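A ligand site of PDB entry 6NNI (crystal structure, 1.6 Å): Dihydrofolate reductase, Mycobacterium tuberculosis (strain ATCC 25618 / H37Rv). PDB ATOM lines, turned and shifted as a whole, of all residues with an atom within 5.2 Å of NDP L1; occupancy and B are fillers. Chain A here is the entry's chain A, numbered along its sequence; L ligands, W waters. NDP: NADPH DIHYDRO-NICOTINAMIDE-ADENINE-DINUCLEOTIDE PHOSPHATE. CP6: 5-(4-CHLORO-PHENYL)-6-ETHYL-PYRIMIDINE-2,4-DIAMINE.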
ATOM      1  N   ILE A   5      12.295  11.025 -23.235  1.00  0.00           N
ATOM      2  CA  ILE A   5      11.373  12.051 -23.732  1.00  0.00           C
ATOM      3  C   ILE A   5      12.189  13.101 -24.489  1.00  0.00           C
ATOM      4  O   ILE A   5      13.210  13.592 -23.984  1.00  0.00           O
ATOM      5  CB  ILE A   5      10.529  12.666 -22.587  1.00  0.00           C
ATOM      6  CG1 ILE A   5       9.527  13.685 -23.147  1.00  0.00           C
ATOM      7  CG2 ILE A   5      11.406  13.239 -21.462  1.00  0.00           C
ATOM      8  CD1 ILE A   5       8.384  14.018 -22.152  1.00  0.00           C
ATOM      9  N   TRP A   6      11.758  13.392 -25.715  1.00  0.00           N
ATOM     10  CA  TRP A   6      12.489  14.349 -26.556  1.00  0.00           C
ATOM     11  C   TRP A   6      11.546  14.957 -27.571  1.00  0.00           C
ATOM     12  O   TRP A   6      10.482  14.415 -27.865  1.00  0.00           O
ATOM     13  CB  TRP A   6      13.685  13.688 -27.271  1.00  0.00           C
ATOM     14  CG  TRP A   6      13.363  12.768 -28.417  1.00  0.00           C
ATOM     15  CD1 TRP A   6      13.053  13.129 -29.705  1.00  0.00           C
ATOM     16  CD2 TRP A   6      13.358  11.331 -28.407  1.00  0.00           C
ATOM     17  NE1 TRP A   6      12.845  12.009 -30.484  1.00  0.00           N
ATOM     18  CE2 TRP A   6      13.041  10.900 -29.703  1.00  0.00           C
ATOM     19  CE3 TRP A   6      13.615  10.373 -27.414  1.00  0.00           C
ATOM     20  CZ2 TRP A   6      12.945   9.555 -30.036  1.00  0.00           C
ATOM     21  CZ3 TRP A   6      13.527   9.031 -27.750  1.00  0.00           C
ATOM     22  CH2 TRP A   6      13.195   8.636 -29.057  1.00  0.00           C
ATOM     23  N   ALA A   7      11.958  16.104 -28.106  1.00  0.00           N
ATOM     24  CA  ALA A   7      11.294  16.714 -29.235  1.00  0.00           C
ATOM     25  C   ALA A   7      12.281  16.718 -30.397  1.00  0.00           C
ATOM     26  O   ALA A   7      13.457  17.035 -30.201  1.00  0.00           O
ATOM     27  CB  ALA A   7      10.843  18.146 -28.903  1.00  0.00           C
ATOM     28  N   GLN A   8      11.820  16.323 -31.578  1.00  0.00           N
ATOM     29  CA  GLN A   8      12.693  16.287 -32.747  1.00  0.00           C
ATOM     30  C   GLN A   8      12.045  16.990 -33.928  1.00  0.00           C
ATOM     31  O   GLN A   8      10.819  17.002 -34.072  1.00  0.00           O
ATOM     32  CB  GLN A   8      13.016  14.847 -33.151  1.00  0.00           C
ATOM     33  CG  GLN A   8      11.796  14.059 -33.604  1.00  0.00           C
ATOM     34  CD  GLN A   8      12.197  12.667 -34.083  1.00  0.00           C
ATOM     35  OE1 GLN A   8      12.450  11.772 -33.269  1.00  0.00           O
ATOM     36  NE2 GLN A   8      12.285  12.497 -35.397  1.00  0.00           N
ATOM     37  N   ILE A  14      17.536  16.924 -32.745  1.00  0.00           N
ATOM     38  CA  ILE A  14      17.022  17.394 -31.460  1.00  0.00           C
ATOM     39  C   ILE A  14      17.806  18.589 -30.920  1.00  0.00           C
ATOM     40  O   ILE A  14      17.293  19.291 -30.027  1.00  0.00           O
ATOM     41  CB  ILE A  14      16.988  16.273 -30.398  1.00  0.00           C
ATOM     42  CG1 ILE A  14      18.414  15.814 -30.068  1.00  0.00           C
ATOM     43  CG2 ILE A  14      16.113  15.098 -30.842  1.00  0.00           C
ATOM     44  CD1 ILE A  14      18.489  14.976 -28.793  1.00  0.00           C
ATOM     45  N   GLY A  15      19.012  18.842 -31.386  1.00  0.00           N
ATOM     46  CA  GLY A  15      19.794  19.929 -30.825  1.00  0.00           C
ATOM     47  C   GLY A  15      20.821  20.399 -31.826  1.00  0.00           C
ATOM     48  O   GLY A  15      21.286  19.632 -32.669  1.00  0.00           O
ATOM     49  N   ARG A  16      21.169  21.690 -31.721  1.00  0.00           N
ATOM     50  CA  ARG A  16      22.135  22.307 -32.618  1.00  0.00           C
ATOM     51  C   ARG A  16      22.813  23.452 -31.883  1.00  0.00           C
ATOM     52  O   ARG A  16      22.119  24.261 -31.259  1.00  0.00           O
ATOM     53  CB  ARG A  16      21.429  22.806 -33.880  1.00  0.00           C
ATOM     54  CG  ARG A  16      22.328  23.587 -34.811  1.00  0.00           C
ATOM     55  CD  ARG A  16      21.612  23.828 -36.136  1.00  0.00           C
ATOM     56  NE  ARG A  16      21.415  22.565 -36.839  1.00  0.00           N
ATOM     57  CZ  ARG A  16      20.726  22.443 -37.973  1.00  0.00           C
ATOM     58  NH1 ARG A  16      20.147  23.505 -38.515  1.00  0.00           N
ATOM     59  NH2 ARG A  16      20.608  21.255 -38.562  1.00  0.00           N
ATOM     60  N   GLY A  17      24.136  23.530 -31.980  1.00  0.00           N
ATOM     61  CA  GLY A  17      24.878  24.592 -31.320  1.00  0.00           C
ATOM     62  C   GLY A  17      24.752  24.627 -29.819  1.00  0.00           C
ATOM     63  O   GLY A  17      24.997  25.662 -29.207  1.00  0.00           O
ATOM     64  N   GLY A  18      24.442  23.479 -29.201  1.00  0.00           N
ATOM     65  CA  GLY A  18      24.218  23.419 -27.768  1.00  0.00           C
ATOM     66  C   GLY A  18      22.866  23.881 -27.286  1.00  0.00           C
ATOM     67  O   GLY A  18      22.647  23.978 -26.072  1.00  0.00           O
ATOM     68  N   ASP A  19      21.935  24.163 -28.199  1.00  0.00           N
ATOM     69  CA  ASP A  19      20.578  24.576 -27.852  1.00  0.00           C
ATOM     70  C   ASP A  19      19.627  23.899 -28.826  1.00  0.00           C
ATOM     71  O   ASP A  19      19.940  22.857 -29.406  1.00  0.00           O
ATOM     72  CB  ASP A  19      20.434  26.100 -27.799  1.00  0.00           C
ATOM     73  CG  ASP A  19      19.346  26.524 -26.844  1.00  0.00           C
ATOM     74  OD1 ASP A  19      18.162  26.581 -27.262  1.00  0.00           O
ATOM     75  OD2 ASP A  19      19.666  26.750 -25.645  1.00  0.00           O
ATOM     76  N   ILE A  20      18.407  24.429 -28.931  1.00  0.00           N
ATOM     77  CA  ILE A  20      17.338  23.850 -29.732  1.00  0.00           C
ATOM     78  C   ILE A  20      16.790  24.888 -30.707  1.00  0.00           C
ATOM     79  O   ILE A  20      16.535  26.016 -30.277  1.00  0.00           O
ATOM     80  CB  ILE A  20      16.227  23.320 -28.818  1.00  0.00           C
ATOM     81  CG1 ILE A  20      16.813  22.337 -27.786  1.00  0.00           C
ATOM     82  CG2 ILE A  20      15.111  22.628 -29.628  1.00  0.00           C
ATOM     83  CD1 ILE A  20      15.834  22.015 -26.691  1.00  0.00           C
ATOM     84  N   TRP A  22      14.011  25.682 -32.028  1.00  0.00           N
ATOM     85  CA  TRP A  22      12.575  25.952 -31.957  1.00  0.00           C
ATOM     86  C   TRP A  22      12.218  26.035 -30.487  1.00  0.00           C
ATOM     87  O   TRP A  22      13.033  25.735 -29.623  1.00  0.00           O
ATOM     88  CB  TRP A  22      11.733  24.869 -32.659  1.00  0.00           C
ATOM     89  CG  TRP A  22      11.873  23.510 -31.964  1.00  0.00           C
ATOM     90  CD1 TRP A  22      11.262  23.106 -30.807  1.00  0.00           C
ATOM     91  CD2 TRP A  22      12.680  22.419 -32.398  1.00  0.00           C
ATOM     92  NE1 TRP A  22      11.668  21.823 -30.474  1.00  0.00           N
ATOM     93  CE2 TRP A  22      12.538  21.390 -31.442  1.00  0.00           C
ATOM     94  CE3 TRP A  22      13.540  22.222 -33.478  1.00  0.00           C
ATOM     95  CZ2 TRP A  22      13.194  20.162 -31.557  1.00  0.00           C
ATOM     96  CZ3 TRP A  22      14.188  21.011 -33.598  1.00  0.00           C
ATOM     97  CH2 TRP A  22      14.024  19.998 -32.630  1.00  0.00           C
ATOM     98  N   GLY A  43      22.389  14.652 -19.738  1.00  0.00           N
ATOM     99  CA  GLY A  43      23.820  14.790 -19.912  1.00  0.00           C
ATOM    100  C   GLY A  43      24.310  16.160 -19.456  1.00  0.00           C
ATOM    101  O   GLY A  43      23.548  17.120 -19.372  1.00  0.00           O
ATOM    102  N   ARG A  44      25.612  16.229 -19.177  1.00  0.00           N
ATOM    103  CA  ARG A  44      26.167  17.475 -18.658  1.00  0.00           C
ATOM    104  C   ARG A  44      25.953  18.636 -19.632  1.00  0.00           C
ATOM    105  O   ARG A  44      25.686  19.758 -19.208  1.00  0.00           O
ATOM    106  CB  ARG A  44      27.651  17.288 -18.330  1.00  0.00           C
ATOM    107  CG  ARG A  44      28.291  18.446 -17.567  1.00  0.00           C
ATOM    108  CD  ARG A  44      28.897  19.490 -18.507  1.00  0.00           C
ATOM    109  NE  ARG A  44      29.883  18.890 -19.408  1.00  0.00           N
ATOM    110  CZ  ARG A  44      30.374  19.488 -20.484  1.00  0.00           C
ATOM    111  NH1 ARG A  44      29.973  20.713 -20.796  1.00  0.00           N
ATOM    112  NH2 ARG A  44      31.269  18.866 -21.240  1.00  0.00           N
ATOM    113  N   ARG A  45      26.029  18.373 -20.940  1.00  0.00           N
ATOM    114  CA  ARG A  45      25.813  19.460 -21.896  1.00  0.00           C
ATOM    115  C   ARG A  45      24.383  19.977 -21.835  1.00  0.00           C
ATOM    116  O   ARG A  45      24.145  21.167 -22.080  1.00  0.00           O
ATOM    117  CB  ARG A  45      26.146  18.999 -23.311  1.00  0.00           C
ATOM    118  CG  ARG A  45      27.617  18.654 -23.550  1.00  0.00           C
ATOM    119  CD  ARG A  45      27.811  18.414 -25.045  1.00  0.00           C
ATOM    120  NE  ARG A  45      29.165  18.031 -25.403  1.00  0.00           N
ATOM    121  CZ  ARG A  45      29.469  17.399 -26.531  1.00  0.00           C
ATOM    122  NH1 ARG A  45      30.730  17.081 -26.788  1.00  0.00           N
ATOM    123  NH2 ARG A  45      28.515  17.076 -27.399  1.00  0.00           N
ATOM    124  N   THR A  46      23.418  19.093 -21.557  1.00  0.00           N
ATOM    125  CA  THR A  46      22.034  19.531 -21.446  1.00  0.00           C
ATOM    126  C   THR A  46      21.814  20.342 -20.167  1.00  0.00           C
ATOM    127  O   THR A  46      21.088  21.348 -20.178  1.00  0.00           O
ATOM    128  CB  THR A  46      21.115  18.322 -21.530  1.00  0.00           C
ATOM    129  OG1 THR A  46      21.191  17.783 -22.863  1.00  0.00           O
ATOM    130  CG2 THR A  46      19.660  18.689 -21.237  1.00  0.00           C
ATOM    131  N   SER A  49      22.929  23.793 -20.832  1.00  0.00           N
ATOM    132  CA  SER A  49      22.010  24.578 -21.646  1.00  0.00           C
ATOM    133  C   SER A  49      20.921  25.258 -20.824  1.00  0.00           C
ATOM    134  O   SER A  49      20.260  26.159 -21.334  1.00  0.00           O
ATOM    135  CB  SER A  49      21.375  23.696 -22.729  1.00  0.00           C
ATOM    136  OG  SER A  49      20.310  22.933 -22.214  1.00  0.00           O
ATOM    137  N   LEU A  65      24.663  13.422 -15.800  1.00  0.00           N
ATOM    138  CA  LEU A  65      25.702  12.450 -16.125  1.00  0.00           C
ATOM    139  C   LEU A  65      26.943  13.174 -16.654  1.00  0.00           C
ATOM    140  O   LEU A  65      26.862  13.963 -17.597  1.00  0.00           O
ATOM    141  CB  LEU A  65      25.172  11.467 -17.167  1.00  0.00           C
ATOM    142  CG  LEU A  65      26.144  10.406 -17.671  1.00  0.00           C
ATOM    143  CD1 LEU A  65      26.526   9.456 -16.561  1.00  0.00           C
ATOM    144  CD2 LEU A  65      25.508   9.653 -18.817  1.00  0.00           C
ATOM    145  N   SER A  66      28.096  12.890 -16.026  1.00  0.00           N
ATOM    146  CA  SER A  66      29.367  13.511 -16.399  1.00  0.00           C
ATOM    147  C   SER A  66      30.494  12.544 -16.096  1.00  0.00           C
ATOM    148  O   SER A  66      30.419  11.770 -15.136  1.00  0.00           O
ATOM    149  CB  SER A  66      29.620  14.814 -15.639  1.00  0.00           C
ATOM    150  OG  SER A  66      30.869  15.405 -16.006  1.00  0.00           O
ATOM    151  N   ARG A  67      31.554  12.596 -16.908  1.00  0.00           N
ATOM    152  CA  ARG A  67      32.782  11.874 -16.608  1.00  0.00           C
ATOM    153  C   ARG A  67      33.663  12.615 -15.616  1.00  0.00           C
ATOM    154  O   ARG A  67      34.632  12.031 -15.096  1.00  0.00           O
ATOM    155  CB  ARG A  67      33.583  11.629 -17.896  1.00  0.00           C
ATOM    156  CG  ARG A  67      32.967  10.591 -18.835  1.00  0.00           C
ATOM    157  CD  ARG A  67      33.870  10.378 -20.043  1.00  0.00           C
ATOM    158  NE  ARG A  67      33.294   9.450 -21.015  1.00  0.00           N
ATOM    159  CZ  ARG A  67      32.640   9.838 -22.104  1.00  0.00           C
ATOM    160  NH1 ARG A  67      32.480  11.133 -22.379  1.00  0.00           N
ATOM    161  NH2 ARG A  67      32.147   8.920 -22.925  1.00  0.00           N
ATOM    162  N   GLN A  68      33.353  13.878 -15.347  1.00  0.00           N
ATOM    163  CA  GLN A  68      34.134  14.722 -14.434  1.00  0.00           C
ATOM    164  C   GLN A  68      33.788  14.387 -12.991  1.00  0.00           C
ATOM    165  O   GLN A  68      32.661  14.635 -12.545  1.00  0.00           O
ATOM    166  CB  GLN A  68      33.893  16.199 -14.735  1.00  0.00           C
ATOM    167  CG  GLN A  68      33.935  16.548 -16.219  1.00  0.00           C
ATOM    168  CD  GLN A  68      33.741  18.028 -16.457  1.00  0.00           C
ATOM    169  OE1 GLN A  68      34.375  18.863 -15.799  1.00  0.00           O
ATOM    170  NE2 GLN A  68      32.862  18.377 -17.410  1.00  0.00           N
ATOM    171  N   GLY A  80      28.538   9.381 -12.458  1.00  0.00           N
ATOM    172  CA  GLY A  80      29.509   9.037 -13.468  1.00  0.00           C
ATOM    173  C   GLY A  80      29.061   7.877 -14.340  1.00  0.00           C
ATOM    174  O   GLY A  80      29.726   7.563 -15.329  1.00  0.00           O
ATOM    175  N   SER A  81      27.939   7.259 -13.988  1.00  0.00           N
ATOM    176  CA  SER A  81      27.330   6.230 -14.821  1.00  0.00           C
ATOM    177  C   SER A  81      25.817   6.355 -14.750  1.00  0.00           C
ATOM    178  O   SER A  81      25.250   6.806 -13.743  1.00  0.00           O
ATOM    179  CB  SER A  81      27.750   4.823 -14.387  1.00  0.00           C
ATOM    180  OG  SER A  81      27.123   4.486 -13.164  1.00  0.00           O
ATOM    181  N   ILE A  94      16.061  12.884 -20.205  1.00  0.00           N
ATOM    182  CA  ILE A  94      15.555  14.079 -20.875  1.00  0.00           C
ATOM    183  C   ILE A  94      16.549  14.645 -21.882  1.00  0.00           C
ATOM    184  O   ILE A  94      16.323  15.740 -22.415  1.00  0.00           O
ATOM    185  CB  ILE A  94      15.129  15.137 -19.847  1.00  0.00           C
ATOM    186  CG1 ILE A  94      16.321  15.703 -19.087  1.00  0.00           C
ATOM    187  CG2 ILE A  94      14.100  14.540 -18.896  1.00  0.00           C
ATOM    188  CD1 ILE A  94      16.030  17.096 -18.451  1.00  0.00           C
ATOM    189  N   GLY A  95      17.635  13.929 -22.166  1.00  0.00           N
ATOM    190  CA  GLY A  95      18.576  14.264 -23.234  1.00  0.00           C
ATOM    191  C   GLY A  95      19.963  14.509 -22.692  1.00  0.00           C
ATOM    192  O   GLY A  95      20.203  14.466 -21.487  1.00  0.00           O
ATOM    193  N   GLY A  96      20.895  14.825 -23.605  1.00  0.00           N
ATOM    194  CA  GLY A  96      20.649  14.953 -25.030  1.00  0.00           C
ATOM    195  C   GLY A  96      21.006  13.702 -25.830  1.00  0.00           C
ATOM    196  O   GLY A  96      20.711  12.581 -25.427  1.00  0.00           O
ATOM    197  N   GLY A  97      21.599  13.924 -27.009  1.00  0.00           N
ATOM    198  CA  GLY A  97      21.803  12.840 -27.942  1.00  0.00           C
ATOM    199  C   GLY A  97      22.658  11.710 -27.386  1.00  0.00           C
ATOM    200  O   GLY A  97      22.315  10.535 -27.526  1.00  0.00           O
ATOM    201  N   GLN A  98      23.789  12.058 -26.755  1.00  0.00           N
ATOM    202  CA  GLN A  98      24.657  11.009 -26.213  1.00  0.00           C
ATOM    203  C   GLN A  98      23.935  10.207 -25.146  1.00  0.00           C
ATOM    204  O   GLN A  98      24.046   8.975 -25.104  1.00  0.00           O
ATOM    205  CB  GLN A  98      25.924  11.638 -25.632  1.00  0.00           C
ATOM    206  CG  GLN A  98      26.778  12.334 -26.683  1.00  0.00           C
ATOM    207  CD  GLN A  98      28.048  12.905 -26.114  1.00  0.00           C
ATOM    208  OE1 GLN A  98      28.497  12.515 -25.032  1.00  0.00           O
ATOM    209  NE2 GLN A  98      28.642  13.859 -26.826  1.00  0.00           N
ATOM    210  N   VAL A  99      23.196  10.886 -24.268  1.00  0.00           N
ATOM    211  CA  VAL A  99      22.578  10.162 -23.162  1.00  0.00           C
ATOM    212  C   VAL A  99      21.395   9.307 -23.633  1.00  0.00           C
ATOM    213  O   VAL A  99      21.180   8.224 -23.090  1.00  0.00           O
ATOM    214  CB  VAL A  99      22.210  11.138 -22.029  1.00  0.00           C
ATOM    215  CG1 VAL A  99      21.465  10.395 -20.913  1.00  0.00           C
ATOM    216  CG2 VAL A  99      23.470  11.739 -21.458  1.00  0.00           C
ATOM    217  N   TYR A 100      20.620   9.740 -24.650  1.00  0.00           N
ATOM    218  CA  TYR A 100      19.594   8.846 -25.184  1.00  0.00           C
ATOM    219  C   TYR A 100      20.194   7.548 -25.678  1.00  0.00           C
ATOM    220  O   TYR A 100      19.628   6.473 -25.460  1.00  0.00           O
ATOM    221  CB  TYR A 100      18.818   9.490 -26.339  1.00  0.00           C
ATOM    222  CG  TYR A 100      17.950  10.657 -25.939  1.00  0.00           C
ATOM    223  CD1 TYR A 100      17.132  10.603 -24.817  1.00  0.00           C
ATOM    224  CD2 TYR A 100      17.962  11.833 -26.683  1.00  0.00           C
ATOM    225  CE1 TYR A 100      16.352  11.680 -24.439  1.00  0.00           C
ATOM    226  CE2 TYR A 100      17.211  12.921 -26.307  1.00  0.00           C
ATOM    227  CZ  TYR A 100      16.393  12.839 -25.208  1.00  0.00           C
ATOM    228  OH  TYR A 100      15.675  13.935 -24.856  1.00  0.00           O
ATOM    229  N   LEU A 102      22.891   6.068 -24.687  1.00  0.00           N
ATOM    230  CA  LEU A 102      23.336   5.277 -23.546  1.00  0.00           C
ATOM    231  C   LEU A 102      22.159   4.662 -22.802  1.00  0.00           C
ATOM    232  O   LEU A 102      22.268   3.551 -22.262  1.00  0.00           O
ATOM    233  CB  LEU A 102      24.158   6.155 -22.615  1.00  0.00           C
ATOM    234  CG  LEU A 102      24.759   5.524 -21.381  1.00  0.00           C
ATOM    235  CD1 LEU A 102      25.938   4.644 -21.761  1.00  0.00           C
ATOM    236  CD2 LEU A 102      25.171   6.605 -20.412  1.00  0.00           C
ATOM    237  N   ALA A 126      22.832  17.125 -32.424  1.00  0.00           N
ATOM    238  CA  ALA A 126      22.348  16.004 -31.633  1.00  0.00           C
ATOM    239  C   ALA A 126      21.111  15.421 -32.296  1.00  0.00           C
ATOM    240  O   ALA A 126      20.279  16.150 -32.835  1.00  0.00           O
ATOM    241  CB  ALA A 126      22.045  16.406 -30.192  1.00  0.00           C
HETATM  242  PA  NDP L   1      24.419  15.364 -23.755  1.00  0.00           P
HETATM  243  O1A NDP L   1      23.413  16.305 -23.183  1.00  0.00           O
HETATM  244  O2A NDP L   1      24.049  13.967 -24.134  1.00  0.00           O
HETATM  245  O5B NDP L   1      25.620  15.425 -22.632  1.00  0.00           O
HETATM  246  C5B NDP L   1      26.839  14.855 -23.134  1.00  0.00           C
HETATM  247  C4B NDP L   1      27.732  14.737 -21.886  1.00  0.00           C
HETATM  248  O4B NDP L   1      27.242  13.665 -21.069  1.00  0.00           O
HETATM  249  C3B NDP L   1      29.221  14.427 -22.189  1.00  0.00           C
HETATM  250  O3B NDP L   1      29.925  15.600 -22.518  1.00  0.00           O
HETATM  251  C2B NDP L   1      29.653  13.917 -20.777  1.00  0.00           C
HETATM  252  O2B NDP L   1      29.721  14.860 -19.844  1.00  0.00           O
HETATM  253  C1B NDP L   1      28.390  13.063 -20.403  1.00  0.00           C
HETATM  254  N9A NDP L   1      28.533  11.727 -20.885  1.00  0.00           N
HETATM  255  C8A NDP L   1      28.335  11.228 -22.167  1.00  0.00           C
HETATM  256  N7A NDP L   1      28.603   9.905 -22.256  1.00  0.00           N
HETATM  257  C5A NDP L   1      28.994   9.548 -20.960  1.00  0.00           C
HETATM  258  C6A NDP L   1      29.400   8.329 -20.385  1.00  0.00           C
HETATM  259  N6A NDP L   1      29.460   7.173 -21.148  1.00  0.00           N
HETATM  260  N1A NDP L   1      29.733   8.257 -19.062  1.00  0.00           N
HETATM  261  C2A NDP L   1      29.651   9.431 -18.367  1.00  0.00           C
HETATM  262  N3A NDP L   1      29.268  10.663 -18.764  1.00  0.00           N
HETATM  263  C4A NDP L   1      28.963  10.677 -20.095  1.00  0.00           C
HETATM  264  O3  NDP L   1      25.150  16.223 -25.002  1.00  0.00           O
HETATM  265  PN  NDP L   1      24.595  16.180 -26.517  1.00  0.00           P
HETATM  266  O1N NDP L   1      25.471  17.185 -27.163  1.00  0.00           O
HETATM  267  O2N NDP L   1      24.441  14.809 -27.146  1.00  0.00           O
HETATM  268  O5D NDP L   1      22.988  16.811 -26.496  1.00  0.00           O
HETATM  269  C5D NDP L   1      22.977  18.169 -26.193  1.00  0.00           C
HETATM  270  C4D NDP L   1      22.116  18.844 -27.258  1.00  0.00           C
HETATM  271  O4D NDP L   1      20.803  18.258 -27.231  1.00  0.00           O
HETATM  272  C3D NDP L   1      21.935  20.339 -26.961  1.00  0.00           C
HETATM  273  O3D NDP L   1      21.835  20.957 -28.221  1.00  0.00           O
HETATM  274  C2D NDP L   1      20.579  20.380 -26.246  1.00  0.00           C
HETATM  275  O2D NDP L   1      19.926  21.623 -26.415  1.00  0.00           O
HETATM  276  C1D NDP L   1      19.838  19.301 -27.055  1.00  0.00           C
HETATM  277  N1N NDP L   1      18.676  18.734 -26.322  1.00  0.00           N
HETATM  278  C2N NDP L   1      17.462  18.647 -26.976  1.00  0.00           C
HETATM  279  C3N NDP L   1      16.433  17.924 -26.453  1.00  0.00           C
HETATM  280  C7N NDP L   1      15.156  17.845 -27.147  1.00  0.00           C
HETATM  281  O7N NDP L   1      14.216  17.180 -26.717  1.00  0.00           O
HETATM  282  N7N NDP L   1      14.959  18.554 -28.326  1.00  0.00           N
HETATM  283  C4N NDP L   1      16.584  17.212 -25.170  1.00  0.00           C
HETATM  284  C5N NDP L   1      17.838  17.551 -24.439  1.00  0.00           C
HETATM  285  C6N NDP L   1      18.816  18.274 -25.002  1.00  0.00           C
HETATM  286  P2B NDP L   1      31.338  15.533 -19.503  1.00  0.00           P
HETATM  287  O1X NDP L   1      30.990  16.494 -18.415  1.00  0.00           O
HETATM  288  O2X NDP L   1      31.754  16.160 -20.847  1.00  0.00           O
HETATM  289  O3X NDP L   1      32.036  14.270 -19.105  1.00  0.00           O
HETATM  290  N1  CP6 L   2      11.551  16.673 -24.378  1.00  0.00           N
HETATM  291  C2  CP6 L   2      10.652  17.422 -24.983  1.00  0.00           C
HETATM  292  C3  CP6 L   2      12.598  17.232 -23.785  1.00  0.00           C
HETATM  293  C4  CP6 L   2      12.765  18.615 -23.799  1.00  0.00           C
HETATM  294  C5  CP6 L   2      11.792  19.352 -24.456  1.00  0.00           C
HETATM  295  N6  CP6 L   2      10.785  18.724 -25.033  1.00  0.00           N
HETATM  296  C7  CP6 L   2      13.853  19.233 -23.140  1.00  0.00           C
HETATM  297  C8  CP6 L   2      13.780  19.370 -21.761  1.00  0.00           C
HETATM  298  C9  CP6 L   2      14.815  19.960 -21.033  1.00  0.00           C
HETATM  299  C10 CP6 L   2      15.934  20.409 -21.718  1.00  0.00           C
HETATM  300  C11 CP6 L   2      16.015  20.287 -23.094  1.00  0.00           C
HETATM  301  C12 CP6 L   2      14.972  19.710 -23.803  1.00  0.00           C
HETATM  302  N13 CP6 L   2      13.546  16.380 -23.142  1.00  0.00           N
HETATM  303  N14 CP6 L   2       9.523  16.814 -25.623  1.00  0.00           N
HETATM  304  C15 CP6 L   2      11.802  20.868 -24.555  1.00  0.00           C
HETATM  305  C16 CP6 L   2      10.597  21.397 -23.774  1.00  0.00           C
HETATM  306 CL1  CP6 L   2      17.240  21.182 -20.793  1.00  0.00          CL
HETATM  307  O   HOH W   1      29.784   5.722 -17.590  1.00  0.00           O
HETATM  308  O   HOH W   2      18.590  22.293 -24.229  1.00  0.00           O
HETATM  309  O   HOH W   3      33.526  13.442 -21.206  1.00  0.00           O
HETATM  310  O   HOH W   4      25.444  19.614 -28.111  1.00  0.00           O
HETATM  311  O   HOH W   5      28.530   8.251 -24.442  1.00  0.00           O
HETATM  312  O   HOH W   6      23.799  20.810 -30.146  1.00  0.00           O
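O1X of NDP L1 sits at hydrogen-bond distance from OG of Ser 66 (2.6 Å). N of Thr 46 sits at hydrogen-bond distance from O1A of NDP L1 (3.2 Å). O1A of NDP L1 is in hydrogen-bond range of OG1 of Thr 46 (2.7 Å). The guanidinium group (NH2) of Arg 44 is in salt-bridge range of an oxygen (O2X) of NDP L1. N of Arg 67 sits at hydrogen-bond distance from O3X of NDP L1. NE2 of Gln 68 is in hydrogen-bond range of O1X of NDP L1, at 2.8 Å. An oxygen (O7N) of NDP L1 sits at hydrogen-bond distance from the backbone NH (N) of Ala 7 (2.9 Å). A nitrogen (N7N) of NDP L1 lies within hydrogen-bond range of the backbone carbonyl oxygen of Ala 7, 2.8 Å away. N of Gln 98 lies within hydrogen-bond range of O2N of NDP L1 (2.9 Å). An oxygen (O3D) of NDP L1 is in hydrogen-bond range of the backbone NH (N) of Asp 19 (3.2 Å). O of Asp 19 is in hydrogen-bond range of O3D of NDP L1 (2.9 Å). An oxygen (O1A) of NDP L1 is in hydrogen-bond range of the backbone NH (N) of Gly 96 (3.0 Å). The backbone NH (N) of Gly 97 sits at hydrogen-bond distance from an oxygen (O2N) of NDP L1, at 3.0 Å. O of Ile 14 lies within hydrogen-bond range of N7N of NDP L1 (3.0 Å). The backbone NH (N) of Arg 45 is in hydrogen-bond range of an oxygen (O5B) of NDP L1 (3.4 Å). An oxygen (O1N) of NDP L1 lies within salt-bridge range of the guanidinium group (NH2) of Arg 45 (3.1 Å). An oxygen (O2A) of NDP L1 lies within hydrogen-bond range of the backbone NH (N) of Val 99. N13 of CP6 L2 sits at hydrogen-bond distance from O of Ile 94 (2.9 Å). O of Trp 6 lies close to N14 of CP6 L2, 3.4 Å away. O of Ile 5 lies within hydrogen-bond range of N13 of CP6 L2 (2.9 Å).
OG of Ser 66 is in hydrogen-bond range of N of Gln 68 (3.0 Å). The side-chain hydroxyl (OG1) of Thr 46 lies within hydrogen-bond range of the backbone NH (N) of Gly 96. The side-chain amide nitrogen of Gln 98 lies close to the guanidinium group of Arg 45, at 3.3 Å. N of Ile 14 lies within hydrogen-bond range of O of Ala 126, 2.9 Å away. OE1 of Gln 8 lies within hydrogen-bond range of NE1 of Trp 6, 2.8 Å away. The backbone carbonyl oxygen (O) of Gly 95 is in hydrogen-bond range of the backbone NH (N) of Gly 43 (2.8 Å). N of Gly 95 lies within hydrogen-bond range of OH of Tyr 100. The backbone carbonyl oxygen (O) of Gly 15 lies within hydrogen-bond range of the backbone NH (N) of Ala 126 (3.0 Å).
CA of Trp 6 touches O7N of NDP L1 (3.3 Å). Gly 15 touches NDP L1. Arg 16 touches NDP L1 (N to O3D, 3.6 Å). C of Gly 18 touches O3D of NDP L1 (3.2 Å). CG1 of Ile 20 touches O2D of NDP L1 (3.5 Å). Gly 43 touches NDP L1 (CA to O5B, 3.3 Å). Leu 65 touches NDP L1 (O to C1B, 3.3 Å). Gly 80 touches NDP L1. Ile 94 touches NDP L1. CA of Gly 95 touches C5N of NDP L1 (3.6 Å). OH of Tyr 100 touches C4N of NDP L1, at 3.4 Å. CB of Ala 126 touches O4D of NDP L1, 3.7 Å away. Hydrophobic or aromatic side chains that line NDP L1: Trp 6, Ile 14, Ile 20, Leu 65, Val 99 and Ala 126. The nearest printed residue that does not touch NDP L1 is Trp 22 (4.02 Å).
Water W2 bridges O2D of NDP L1 (2.6 Å) and OG of Ser 49 (2.7 Å). Water W3 bridges an oxygen (O3X) of NDP L1 (2.7 Å) and the guanidinium group (NH1) of Arg 67 (2.8 Å). Water W1 lies within hydrogen-bond range of O of Gly 80 (2.9 Å) and N1A of NDP L1 (2.9 Å).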
